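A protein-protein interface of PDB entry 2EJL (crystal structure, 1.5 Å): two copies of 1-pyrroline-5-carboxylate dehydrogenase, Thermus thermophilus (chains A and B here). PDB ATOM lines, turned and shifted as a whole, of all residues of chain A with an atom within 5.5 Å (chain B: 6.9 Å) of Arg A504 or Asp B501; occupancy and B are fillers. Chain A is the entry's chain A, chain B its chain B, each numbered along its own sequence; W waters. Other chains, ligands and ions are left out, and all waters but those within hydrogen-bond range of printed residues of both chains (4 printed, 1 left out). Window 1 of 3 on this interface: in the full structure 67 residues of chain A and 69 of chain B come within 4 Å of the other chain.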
ATOM      1  N   TYR A 152       4.482 -18.447  15.591  1.00  0.00           N
ATOM      2  CA  TYR A 152       5.439 -18.698  16.662  1.00  0.00           C
ATOM      3  C   TYR A 152       6.828 -19.098  16.157  1.00  0.00           C
ATOM      4  O   TYR A 152       7.698 -19.451  16.969  1.00  0.00           O
ATOM      5  CB  TYR A 152       4.907 -19.804  17.577  1.00  0.00           C
ATOM      6  CG  TYR A 152       3.694 -19.386  18.377  1.00  0.00           C
ATOM      7  CD1 TYR A 152       2.405 -19.622  17.885  1.00  0.00           C
ATOM      8  CD2 TYR A 152       3.826 -18.749  19.620  1.00  0.00           C
ATOM      9  CE1 TYR A 152       1.278 -19.228  18.591  1.00  0.00           C
ATOM     10  CE2 TYR A 152       2.703 -18.360  20.349  1.00  0.00           C
ATOM     11  CZ  TYR A 152       1.430 -18.608  19.826  1.00  0.00           C
ATOM     12  OH  TYR A 152       0.327 -18.224  20.548  1.00  0.00           O
ATOM     13  N   TYR A 171      10.695 -19.660  20.778  1.00  0.00           N
ATOM     14  CA  TYR A 171       9.953 -20.763  21.366  1.00  0.00           C
ATOM     15  C   TYR A 171      10.473 -22.147  20.955  1.00  0.00           C
ATOM     16  O   TYR A 171      10.956 -22.363  19.830  1.00  0.00           O
ATOM     17  CB  TYR A 171       8.474 -20.622  21.012  1.00  0.00           C
ATOM     18  CG  TYR A 171       7.882 -19.330  21.521  1.00  0.00           C
ATOM     19  CD1 TYR A 171       7.475 -18.313  20.639  1.00  0.00           C
ATOM     20  CD2 TYR A 171       7.745 -19.099  22.896  1.00  0.00           C
ATOM     21  CE1 TYR A 171       6.936 -17.125  21.113  1.00  0.00           C
ATOM     22  CE2 TYR A 171       7.207 -17.909  23.376  1.00  0.00           C
ATOM     23  CZ  TYR A 171       6.794 -16.931  22.474  1.00  0.00           C
ATOM     24  OH  TYR A 171       6.272 -15.740  22.935  1.00  0.00           O
ATOM     25  N   ARG A 284       2.736 -29.333  32.992  1.00  0.00           N
ATOM     26  CA  ARG A 284       1.618 -28.495  32.589  1.00  0.00           C
ATOM     27  C   ARG A 284       0.397 -29.371  32.352  1.00  0.00           C
ATOM     28  O   ARG A 284       0.497 -30.416  31.728  1.00  0.00           O
ATOM     29  CB  ARG A 284       1.943 -27.712  31.315  1.00  0.00           C
ATOM     30  CG  ARG A 284       3.139 -26.793  31.462  1.00  0.00           C
ATOM     31  CD  ARG A 284       3.215 -25.831  30.285  1.00  0.00           C
ATOM     32  NE  ARG A 284       4.398 -24.983  30.381  1.00  0.00           N
ATOM     33  CZ  ARG A 284       4.779 -24.132  29.429  1.00  0.00           C
ATOM     34  NH1 ARG A 284       4.075 -24.002  28.313  1.00  0.00           N
ATOM     35  NH2 ARG A 284       5.884 -23.418  29.589  1.00  0.00           N
ATOM     36  N   LEU A 500      -5.184 -18.259  18.631  1.00  0.00           N
ATOM     37  CA  LEU A 500      -3.729 -18.128  18.593  1.00  0.00           C
ATOM     38  C   LEU A 500      -3.079 -18.540  19.924  1.00  0.00           C
ATOM     39  O   LEU A 500      -2.065 -19.248  19.929  1.00  0.00           O
ATOM     40  CB  LEU A 500      -3.323 -16.700  18.198  1.00  0.00           C
ATOM     41  CG  LEU A 500      -3.685 -16.313  16.765  1.00  0.00           C
ATOM     42  CD1 LEU A 500      -3.533 -14.812  16.562  1.00  0.00           C
ATOM     43  CD2 LEU A 500      -2.828 -17.091  15.779  1.00  0.00           C
ATOM     44  N   ASP A 501      -3.686 -18.116  21.032  1.00  0.00           N
ATOM     45  CA  ASP A 501      -3.142 -18.346  22.376  1.00  0.00           C
ATOM     46  C   ASP A 501      -3.029 -19.818  22.740  1.00  0.00           C
ATOM     47  O   ASP A 501      -2.228 -20.167  23.582  1.00  0.00           O
ATOM     48  CB  ASP A 501      -4.008 -17.660  23.440  1.00  0.00           C
ATOM     49  CG  ASP A 501      -3.769 -16.166  23.529  1.00  0.00           C
ATOM     50  OD1 ASP A 501      -2.948 -15.626  22.752  1.00  0.00           O
ATOM     51  OD2 ASP A 501      -4.444 -15.541  24.380  1.00  0.00           O
ATOM     52  N   TYR A 502      -3.844 -20.684  22.128  1.00  0.00           N
ATOM     53  CA  TYR A 502      -3.775 -22.118  22.464  1.00  0.00           C
ATOM     54  C   TYR A 502      -2.366 -22.682  22.288  1.00  0.00           C
ATOM     55  O   TYR A 502      -1.890 -23.444  23.124  1.00  0.00           O
ATOM     56  CB  TYR A 502      -4.720 -22.901  21.576  1.00  0.00           C
ATOM     57  CG  TYR A 502      -5.070 -24.292  22.046  1.00  0.00           C
ATOM     58  CD1 TYR A 502      -5.715 -24.503  23.262  1.00  0.00           C
ATOM     59  CD2 TYR A 502      -4.819 -25.397  21.230  1.00  0.00           C
ATOM     60  CE1 TYR A 502      -6.074 -25.790  23.672  1.00  0.00           C
ATOM     61  CE2 TYR A 502      -5.196 -26.695  21.618  1.00  0.00           C
ATOM     62  CZ  TYR A 502      -5.811 -26.888  22.841  1.00  0.00           C
ATOM     63  OH  TYR A 502      -6.193 -28.173  23.209  1.00  0.00           O
ATOM     64  N   LEU A 503      -1.706 -22.343  21.178  1.00  0.00           N
ATOM     65  CA  LEU A 503      -0.421 -22.978  20.908  1.00  0.00           C
ATOM     66  C   LEU A 503       0.686 -22.560  21.877  1.00  0.00           C
ATOM     67  O   LEU A 503       1.624 -23.336  22.114  1.00  0.00           O
ATOM     68  CB  LEU A 503       0.003 -22.783  19.453  1.00  0.00           C
ATOM     69  CG  LEU A 503      -1.024 -23.278  18.420  1.00  0.00           C
ATOM     70  CD1 LEU A 503      -0.424 -23.117  17.043  1.00  0.00           C
ATOM     71  CD2 LEU A 503      -1.442 -24.722  18.661  1.00  0.00           C
ATOM     72  N   ARG A 504       0.557 -21.367  22.459  1.00  0.00           N
ATOM     73  CA  ARG A 504       1.552 -20.872  23.397  1.00  0.00           C
ATOM     74  C   ARG A 504       1.656 -21.786  24.624  1.00  0.00           C
ATOM     75  O   ARG A 504       2.723 -21.866  25.248  1.00  0.00           O
ATOM     76  CB  ARG A 504       1.200 -19.442  23.817  1.00  0.00           C
ATOM     77  CG  ARG A 504       2.207 -18.799  24.759  1.00  0.00           C
ATOM     78  CD  ARG A 504       3.614 -18.751  24.184  1.00  0.00           C
ATOM     79  NE  ARG A 504       4.568 -18.174  25.137  1.00  0.00           N
ATOM     80  CZ  ARG A 504       5.209 -18.847  26.089  1.00  0.00           C
ATOM     81  NH1 ARG A 504       6.056 -18.190  26.871  1.00  0.00           N
ATOM     82  NH2 ARG A 504       5.010 -20.155  26.269  1.00  0.00           N
ATOM     83  N   LEU A 505       0.546 -22.454  24.950  1.00  0.00           N
ATOM     84  CA  LEU A 505       0.482 -23.367  26.087  1.00  0.00           C
ATOM     85  C   LEU A 505       1.437 -24.555  25.945  1.00  0.00           C
ATOM     86  O   LEU A 505       1.799 -25.206  26.942  1.00  0.00           O
ATOM     87  CB  LEU A 505      -0.942 -23.888  26.259  1.00  0.00           C
ATOM     88  CG  LEU A 505      -2.010 -22.838  26.529  1.00  0.00           C
ATOM     89  CD1 LEU A 505      -3.356 -23.534  26.439  1.00  0.00           C
ATOM     90  CD2 LEU A 505      -1.805 -22.167  27.874  1.00  0.00           C
ATOM     91  N   PHE A 506       1.805 -24.854  24.709  1.00  0.00           N
ATOM     92  CA  PHE A 506       2.622 -26.044  24.385  1.00  0.00           C
ATOM     93  C   PHE A 506       4.073 -25.694  23.997  1.00  0.00           C
ATOM     94  O   PHE A 506       4.807 -26.525  23.432  1.00  0.00           O
ATOM     95  CB  PHE A 506       1.954 -26.819  23.234  1.00  0.00           C
ATOM     96  CG  PHE A 506       0.453 -26.903  23.342  1.00  0.00           C
ATOM     97  CD1 PHE A 506      -0.354 -26.569  22.264  1.00  0.00           C
ATOM     98  CD2 PHE A 506      -0.151 -27.285  24.537  1.00  0.00           C
ATOM     99  CE1 PHE A 506      -1.743 -26.652  22.364  1.00  0.00           C
ATOM    100  CE2 PHE A 506      -1.537 -27.360  24.653  1.00  0.00           C
ATOM    101  CZ  PHE A 506      -2.330 -27.039  23.571  1.00  0.00           C
ATOM    102  N   LEU A 507       4.476 -24.463  24.349  1.00  0.00           N
ATOM    103  CA  LEU A 507       5.825 -23.949  24.087  1.00  0.00           C
ATOM    104  C   LEU A 507       6.446 -23.388  25.355  1.00  0.00           C
ATOM    105  O   LEU A 507       5.735 -22.923  26.261  1.00  0.00           O
ATOM    106  CB  LEU A 507       5.760 -22.819  23.060  1.00  0.00           C
ATOM    107  CG  LEU A 507       5.220 -23.166  21.671  1.00  0.00           C
ATOM    108  CD1 LEU A 507       4.863 -21.885  20.893  1.00  0.00           C
ATOM    109  CD2 LEU A 507       6.266 -24.039  20.936  1.00  0.00           C
ATOM    110  N   GLU A 508       7.773 -23.416  25.395  1.00  0.00           N
ATOM    111  CA  GLU A 508       8.549 -22.666  26.383  1.00  0.00           C
ATOM    112  C   GLU A 508       9.509 -21.762  25.615  1.00  0.00           C
ATOM    113  O   GLU A 508       9.781 -21.992  24.431  1.00  0.00           O
ATOM    114  CB  GLU A 508       9.278 -23.574  27.394  1.00  0.00           C
ATOM    115  CG  GLU A 508      10.092 -24.732  26.791  1.00  0.00           C
ATOM    116  CD  GLU A 508      10.506 -25.794  27.829  1.00  0.00           C
ATOM    117  OE1 GLU A 508      10.223 -25.611  29.034  1.00  0.00           O
ATOM    118  OE2 GLU A 508      11.142 -26.797  27.432  1.00  0.00           O
ATOM    119  N   MET A 509      10.027 -20.741  26.290  1.00  0.00           N
ATOM    120  CA  MET A 509      10.860 -19.729  25.631  1.00  0.00           C
ATOM    121  C   MET A 509      12.312 -19.821  26.080  1.00  0.00           C
ATOM    122  O   MET A 509      12.583 -19.996  27.277  1.00  0.00           O
ATOM    123  CB  MET A 509      10.335 -18.329  25.938  1.00  0.00           C
ATOM    124  CG  MET A 509      10.935 -17.237  25.054  1.00  0.00           C
ATOM    125  SD  MET A 509      10.684 -15.564  25.687  1.00  0.00           S
ATOM    126  CE  MET A 509       8.905 -15.375  25.640  1.00  0.00           C
ATOM    127  N   TYR B 144       8.613  -1.281  32.018  1.00  0.00           N
ATOM    128  CA  TYR B 144       8.354  -2.260  30.979  1.00  0.00           C
ATOM    129  C   TYR B 144       6.922  -2.793  31.065  1.00  0.00           C
ATOM    130  O   TYR B 144       6.199  -2.793  30.062  1.00  0.00           O
ATOM    131  CB  TYR B 144       9.375  -3.401  31.048  1.00  0.00           C
ATOM    132  CG  TYR B 144       9.224  -4.387  29.920  1.00  0.00           C
ATOM    133  CD1 TYR B 144       9.942  -4.236  28.740  1.00  0.00           C
ATOM    134  CD2 TYR B 144       8.339  -5.449  30.026  1.00  0.00           C
ATOM    135  CE1 TYR B 144       9.795  -5.142  27.682  1.00  0.00           C
ATOM    136  CE2 TYR B 144       8.172  -6.340  28.998  1.00  0.00           C
ATOM    137  CZ  TYR B 144       8.907  -6.191  27.820  1.00  0.00           C
ATOM    138  OH  TYR B 144       8.765  -7.083  26.769  1.00  0.00           O
ATOM    139  N   ALA B 148       3.923  -2.819  28.391  1.00  0.00           N
ATOM    140  CA  ALA B 148       3.484  -4.118  27.883  1.00  0.00           C
ATOM    141  C   ALA B 148       1.993  -4.353  28.115  1.00  0.00           C
ATOM    142  O   ALA B 148       1.319  -4.974  27.291  1.00  0.00           O
ATOM    143  CB  ALA B 148       4.312  -5.246  28.492  1.00  0.00           C
ATOM    144  N   TYR B 152      -2.285  -5.554  25.708  1.00  0.00           N
ATOM    145  CA  TYR B 152      -3.399  -6.460  26.011  1.00  0.00           C
ATOM    146  C   TYR B 152      -4.745  -5.724  26.144  1.00  0.00           C
ATOM    147  O   TYR B 152      -5.742  -6.341  26.514  1.00  0.00           O
ATOM    148  CB  TYR B 152      -3.097  -7.227  27.310  1.00  0.00           C
ATOM    149  CG  TYR B 152      -1.945  -8.194  27.187  1.00  0.00           C
ATOM    150  CD1 TYR B 152      -0.641  -7.810  27.512  1.00  0.00           C
ATOM    151  CD2 TYR B 152      -2.155  -9.502  26.764  1.00  0.00           C
ATOM    152  CE1 TYR B 152       0.424  -8.704  27.386  1.00  0.00           C
ATOM    153  CE2 TYR B 152      -1.104 -10.406  26.646  1.00  0.00           C
ATOM    154  CZ  TYR B 152       0.184  -9.996  26.971  1.00  0.00           C
ATOM    155  OH  TYR B 152       1.254 -10.853  26.874  1.00  0.00           O
ATOM    156  N   ASN B 494       8.892 -21.465  33.685  1.00  0.00           N
ATOM    157  CA  ASN B 494       9.218 -20.663  32.499  1.00  0.00           C
ATOM    158  C   ASN B 494       8.345 -19.407  32.372  1.00  0.00           C
ATOM    159  O   ASN B 494       7.987 -19.008  31.267  1.00  0.00           O
ATOM    160  CB  ASN B 494       9.139 -21.522  31.220  1.00  0.00           C
ATOM    161  CG  ASN B 494       9.864 -20.897  30.037  1.00  0.00           C
ATOM    162  OD1 ASN B 494       9.245 -20.580  29.020  1.00  0.00           O
ATOM    163  ND2 ASN B 494      11.182 -20.732  30.155  1.00  0.00           N
ATOM    164  N   ALA B 495       8.002 -18.792  33.503  1.00  0.00           N
ATOM    165  CA  ALA B 495       7.295 -17.519  33.470  1.00  0.00           C
ATOM    166  C   ALA B 495       8.351 -16.465  33.186  1.00  0.00           C
ATOM    167  O   ALA B 495       9.149 -16.114  34.062  1.00  0.00           O
ATOM    168  CB  ALA B 495       6.575 -17.259  34.807  1.00  0.00           C
ATOM    169  N   LYS B 496       8.411 -15.992  31.939  1.00  0.00           N
ATOM    170  CA  LYS B 496       9.493 -15.102  31.511  1.00  0.00           C
ATOM    171  C   LYS B 496       9.274 -13.668  31.960  1.00  0.00           C
ATOM    172  O   LYS B 496       8.421 -12.946  31.418  1.00  0.00           O
ATOM    173  CB  LYS B 496       9.691 -15.171  29.991  1.00  0.00           C
ATOM    174  CG  LYS B 496      10.345 -16.457  29.520  1.00  0.00           C
ATOM    175  CD  LYS B 496      11.798 -16.512  29.995  1.00  0.00           C
ATOM    176  CE  LYS B 496      12.712 -17.194  28.975  1.00  0.00           C
ATOM    177  NZ  LYS B 496      14.125 -17.262  29.463  1.00  0.00           N
ATOM    178  N   GLY B 498      10.098  -9.673  32.562  1.00  0.00           N
ATOM    179  CA  GLY B 498      10.615  -8.632  31.665  1.00  0.00           C
ATOM    180  C   GLY B 498      10.374  -8.959  30.202  1.00  0.00           C
ATOM    181  O   GLY B 498      11.165  -8.568  29.332  1.00  0.00           O
ATOM    182  N   ALA B 499       9.256  -9.648  29.944  1.00  0.00           N
ATOM    183  CA  ALA B 499       8.865 -10.029  28.585  1.00  0.00           C
ATOM    184  C   ALA B 499       7.366  -9.798  28.436  1.00  0.00           C
ATOM    185  O   ALA B 499       6.637  -9.906  29.427  1.00  0.00           O
ATOM    186  CB  ALA B 499       9.219 -11.487  28.327  1.00  0.00           C
ATOM    187  N   LEU B 500       6.913  -9.518  27.210  1.00  0.00           N
ATOM    188  CA  LEU B 500       5.479  -9.335  26.922  1.00  0.00           C
ATOM    189  C   LEU B 500       4.642 -10.487  27.454  1.00  0.00           C
ATOM    190  O   LEU B 500       3.556 -10.276  28.013  1.00  0.00           O
ATOM    191  CB  LEU B 500       5.230  -9.204  25.416  1.00  0.00           C
ATOM    192  CG  LEU B 500       5.863  -7.959  24.799  1.00  0.00           C
ATOM    193  CD1 LEU B 500       5.953  -8.080  23.275  1.00  0.00           C
ATOM    194  CD2 LEU B 500       5.101  -6.719  25.192  1.00  0.00           C
ATOM    195  N   ASP B 501       5.163 -11.698  27.295  1.00  0.00           N
ATOM    196  CA  ASP B 501       4.464 -12.928  27.695  1.00  0.00           C
ATOM    197  C   ASP B 501       4.160 -13.020  29.186  1.00  0.00           C
ATOM    198  O   ASP B 501       3.273 -13.764  29.578  1.00  0.00           O
ATOM    199  CB  ASP B 501       5.258 -14.171  27.286  1.00  0.00           C
ATOM    200  CG  ASP B 501       5.093 -14.526  25.818  1.00  0.00           C
ATOM    201  OD1 ASP B 501       4.438 -13.784  25.050  1.00  0.00           O
ATOM    202  OD2 ASP B 501       5.648 -15.563  25.431  1.00  0.00           O
ATOM    203  N   TYR B 502       4.905 -12.300  30.023  1.00  0.00           N
ATOM    204  CA  TYR B 502       4.673 -12.402  31.460  1.00  0.00           C
ATOM    205  C   TYR B 502       3.239 -12.029  31.812  1.00  0.00           C
ATOM    206  O   TYR B 502       2.603 -12.712  32.611  1.00  0.00           O
ATOM    207  CB  TYR B 502       5.638 -11.507  32.213  1.00  0.00           C
ATOM    208  CG  TYR B 502       5.761 -11.745  33.699  1.00  0.00           C
ATOM    209  CD1 TYR B 502       6.272 -12.947  34.193  1.00  0.00           C
ATOM    210  CD2 TYR B 502       5.461 -10.736  34.600  1.00  0.00           C
ATOM    211  CE1 TYR B 502       6.444 -13.145  35.569  1.00  0.00           C
ATOM    212  CE2 TYR B 502       5.631 -10.917  35.976  1.00  0.00           C
ATOM    213  CZ  TYR B 502       6.126 -12.126  36.442  1.00  0.00           C
ATOM    214  OH  TYR B 502       6.308 -12.274  37.803  1.00  0.00           O
ATOM    215  N   LEU B 503       2.730 -10.964  31.198  1.00  0.00           N
ATOM    216  CA  LEU B 503       1.461 -10.413  31.643  1.00  0.00           C
ATOM    217  C   LEU B 503       0.294 -11.333  31.288  1.00  0.00           C
ATOM    218  O   LEU B 503      -0.722 -11.350  31.989  1.00  0.00           O
ATOM    219  CB  LEU B 503       1.263  -8.981  31.129  1.00  0.00           C
ATOM    220  CG  LEU B 503       2.355  -7.990  31.570  1.00  0.00           C
ATOM    221  CD1 LEU B 503       1.996  -6.634  31.049  1.00  0.00           C
ATOM    222  CD2 LEU B 503       2.556  -7.924  33.097  1.00  0.00           C
ATOM    223  N   ARG B 504       0.480 -12.131  30.235  1.00  0.00           N
ATOM    224  CA  ARG B 504      -0.557 -13.039  29.770  1.00  0.00           C
ATOM    225  C   ARG B 504      -0.898 -14.069  30.843  1.00  0.00           C
ATOM    226  O   ARG B 504      -2.022 -14.562  30.902  1.00  0.00           O
ATOM    227  CB  ARG B 504      -0.097 -13.704  28.469  1.00  0.00           C
ATOM    228  CG  ARG B 504      -1.049 -14.725  27.898  1.00  0.00           C
ATOM    229  CD  ARG B 504      -2.351 -14.067  27.485  1.00  0.00           C
ATOM    230  NE  ARG B 504      -3.345 -15.004  26.947  1.00  0.00           N
ATOM    231  CZ  ARG B 504      -4.205 -15.703  27.685  1.00  0.00           C
ATOM    232  NH1 ARG B 504      -5.090 -16.493  27.081  1.00  0.00           N
ATOM    233  NH2 ARG B 504      -4.197 -15.621  29.017  1.00  0.00           N
ATOM    234  N   LEU B 505       0.087 -14.377  31.684  1.00  0.00           N
ATOM    235  CA  LEU B 505      -0.070 -15.342  32.772  1.00  0.00           C
ATOM    236  C   LEU B 505      -1.111 -14.906  33.789  1.00  0.00           C
ATOM    237  O   LEU B 505      -1.672 -15.733  34.520  1.00  0.00           O
ATOM    238  CB  LEU B 505       1.276 -15.575  33.463  1.00  0.00           C
ATOM    239  CG  LEU B 505       2.408 -16.126  32.600  1.00  0.00           C
ATOM    240  CD1 LEU B 505       3.672 -16.142  33.435  1.00  0.00           C
ATOM    241  CD2 LEU B 505       2.062 -17.528  32.113  1.00  0.00           C
ATOM    242  N   PHE B 506      -1.376 -13.602  33.821  1.00  0.00           N
ATOM    243  CA  PHE B 506      -2.241 -13.011  34.843  1.00  0.00           C
ATOM    244  C   PHE B 506      -3.564 -12.540  34.262  1.00  0.00           C
ATOM    245  O   PHE B 506      -4.291 -11.724  34.866  1.00  0.00           O
ATOM    246  CB  PHE B 506      -1.540 -11.809  35.495  1.00  0.00           C
ATOM    247  CG  PHE B 506      -0.078 -12.027  35.769  1.00  0.00           C
ATOM    248  CD1 PHE B 506       0.872 -11.120  35.298  1.00  0.00           C
ATOM    249  CD2 PHE B 506       0.350 -13.137  36.485  1.00  0.00           C
ATOM    250  CE1 PHE B 506       2.220 -11.310  35.563  1.00  0.00           C
ATOM    251  CE2 PHE B 506       1.696 -13.342  36.746  1.00  0.00           C
ATOM    252  CZ  PHE B 506       2.632 -12.429  36.277  1.00  0.00           C
HETATM  253  O   HOH W   1       6.191 -12.959  22.918  1.00  0.00           O
HETATM  254  O   HOH W   2       2.953 -15.822  23.141  1.00  0.00           O
HETATM  255  O   HOH W   3       6.508 -20.626  28.674  1.00  0.00           O
HETATM  256  O   HOH W   4       6.665 -17.005  29.716  1.00  0.00           O
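The side-chain carboxylate of Asp B501 lies within hydrogen-bond range of the side-chain hydroxyl of Tyr A171, at 2.6 Å.
The guanidinium group of Arg B504 is in salt-bridge range of the side-chain carboxylate of Asp A501 (2.8 Å).
The side-chain carboxylate (OD2) of Asp B501 is in salt-bridge range of the guanidinium group (NE) of Arg A504, 2.8 Å away.
The backbone NH (N) of Met A509 is in hydrogen-bond range of the side-chain amide oxygen (OD1) of Asn B494 (2.8 Å).
The backbone carbonyl oxygen (O) of Leu A507 sits at hydrogen-bond distance from the guanidinium group (NH2) of Arg A504, 2.9 Å away.
Among the printed residues, pairs that only touch across the chains: Met A509 with Asp B501 (3.3 Å), Met A509 with Lys B496 (3.3 Å) and Glu A508 with Asn B494 (3.4 Å).
Of the printed residues of chain B, Tyr A171 touches Asp B501.
Printed residues of chain B within 4 Å of Asp A501: Arg B504 (2.8 Å).
Of the printed residues of chain B, Glu A508 touches Asn B494.
Of the printed residues of chain B, Met A509 touches Asn B494 (2.8 Å), Lys B496 (3.3 Å) and Asp B501 (3.3 Å).
Leu B500 touches none of the printed residues of chain A.
Printed residues of chain A within 4 Å of Asp B501: Tyr A171, Arg A504 and Met A509.
The nearest printed residue of chain A that does not touch Asp B501 is Tyr A152 (6.5 Å).
The nearest printed residue of chain A that does not touch Arg B504 is Arg A504 (6.1 Å).
Of the 13 printed residues of chain A, 5 touch a printed residue of chain B.
Among the printed residues, 7 pairs touch across the chains.
Asp A501 touches Arg B504, and with the chains exchanged Arg A504 touches Asp B501.
Positions printed for both chains: 152, 500, 501, 502, 503, 504, 505 and 506.
Water W3 lies within hydrogen-bond range of the side-chain amide oxygen (OD1) of Asn B494 (2.8 Å), the guanidinium group (NH2) of Arg A504 (2.9 Å), the guanidinium group (NH2) of Arg A284 (3.0 Å) and the backbone carbonyl oxygen (O) of Leu A507 (3.4 Å).
Water W1 lies within hydrogen-bond range of OH of Tyr A171 (2.8 Å) and OD1 of Asp B501 (2.9 Å).
Water W4 lies within hydrogen-bond range of O of Asn B494 (2.9 Å), N of Lys B496 (3.0 Å) and NH1 of Arg A504 (3.1 Å).
Water W2 lies within hydrogen-bond range of the side-chain carboxylate (OD1) of Asp B501 (3.2 Å), the side-chain hydroxyl (OH) of Tyr A171 (3.3 Å) and the guanidinium group (NE) of Arg A504 (3.5 Å).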
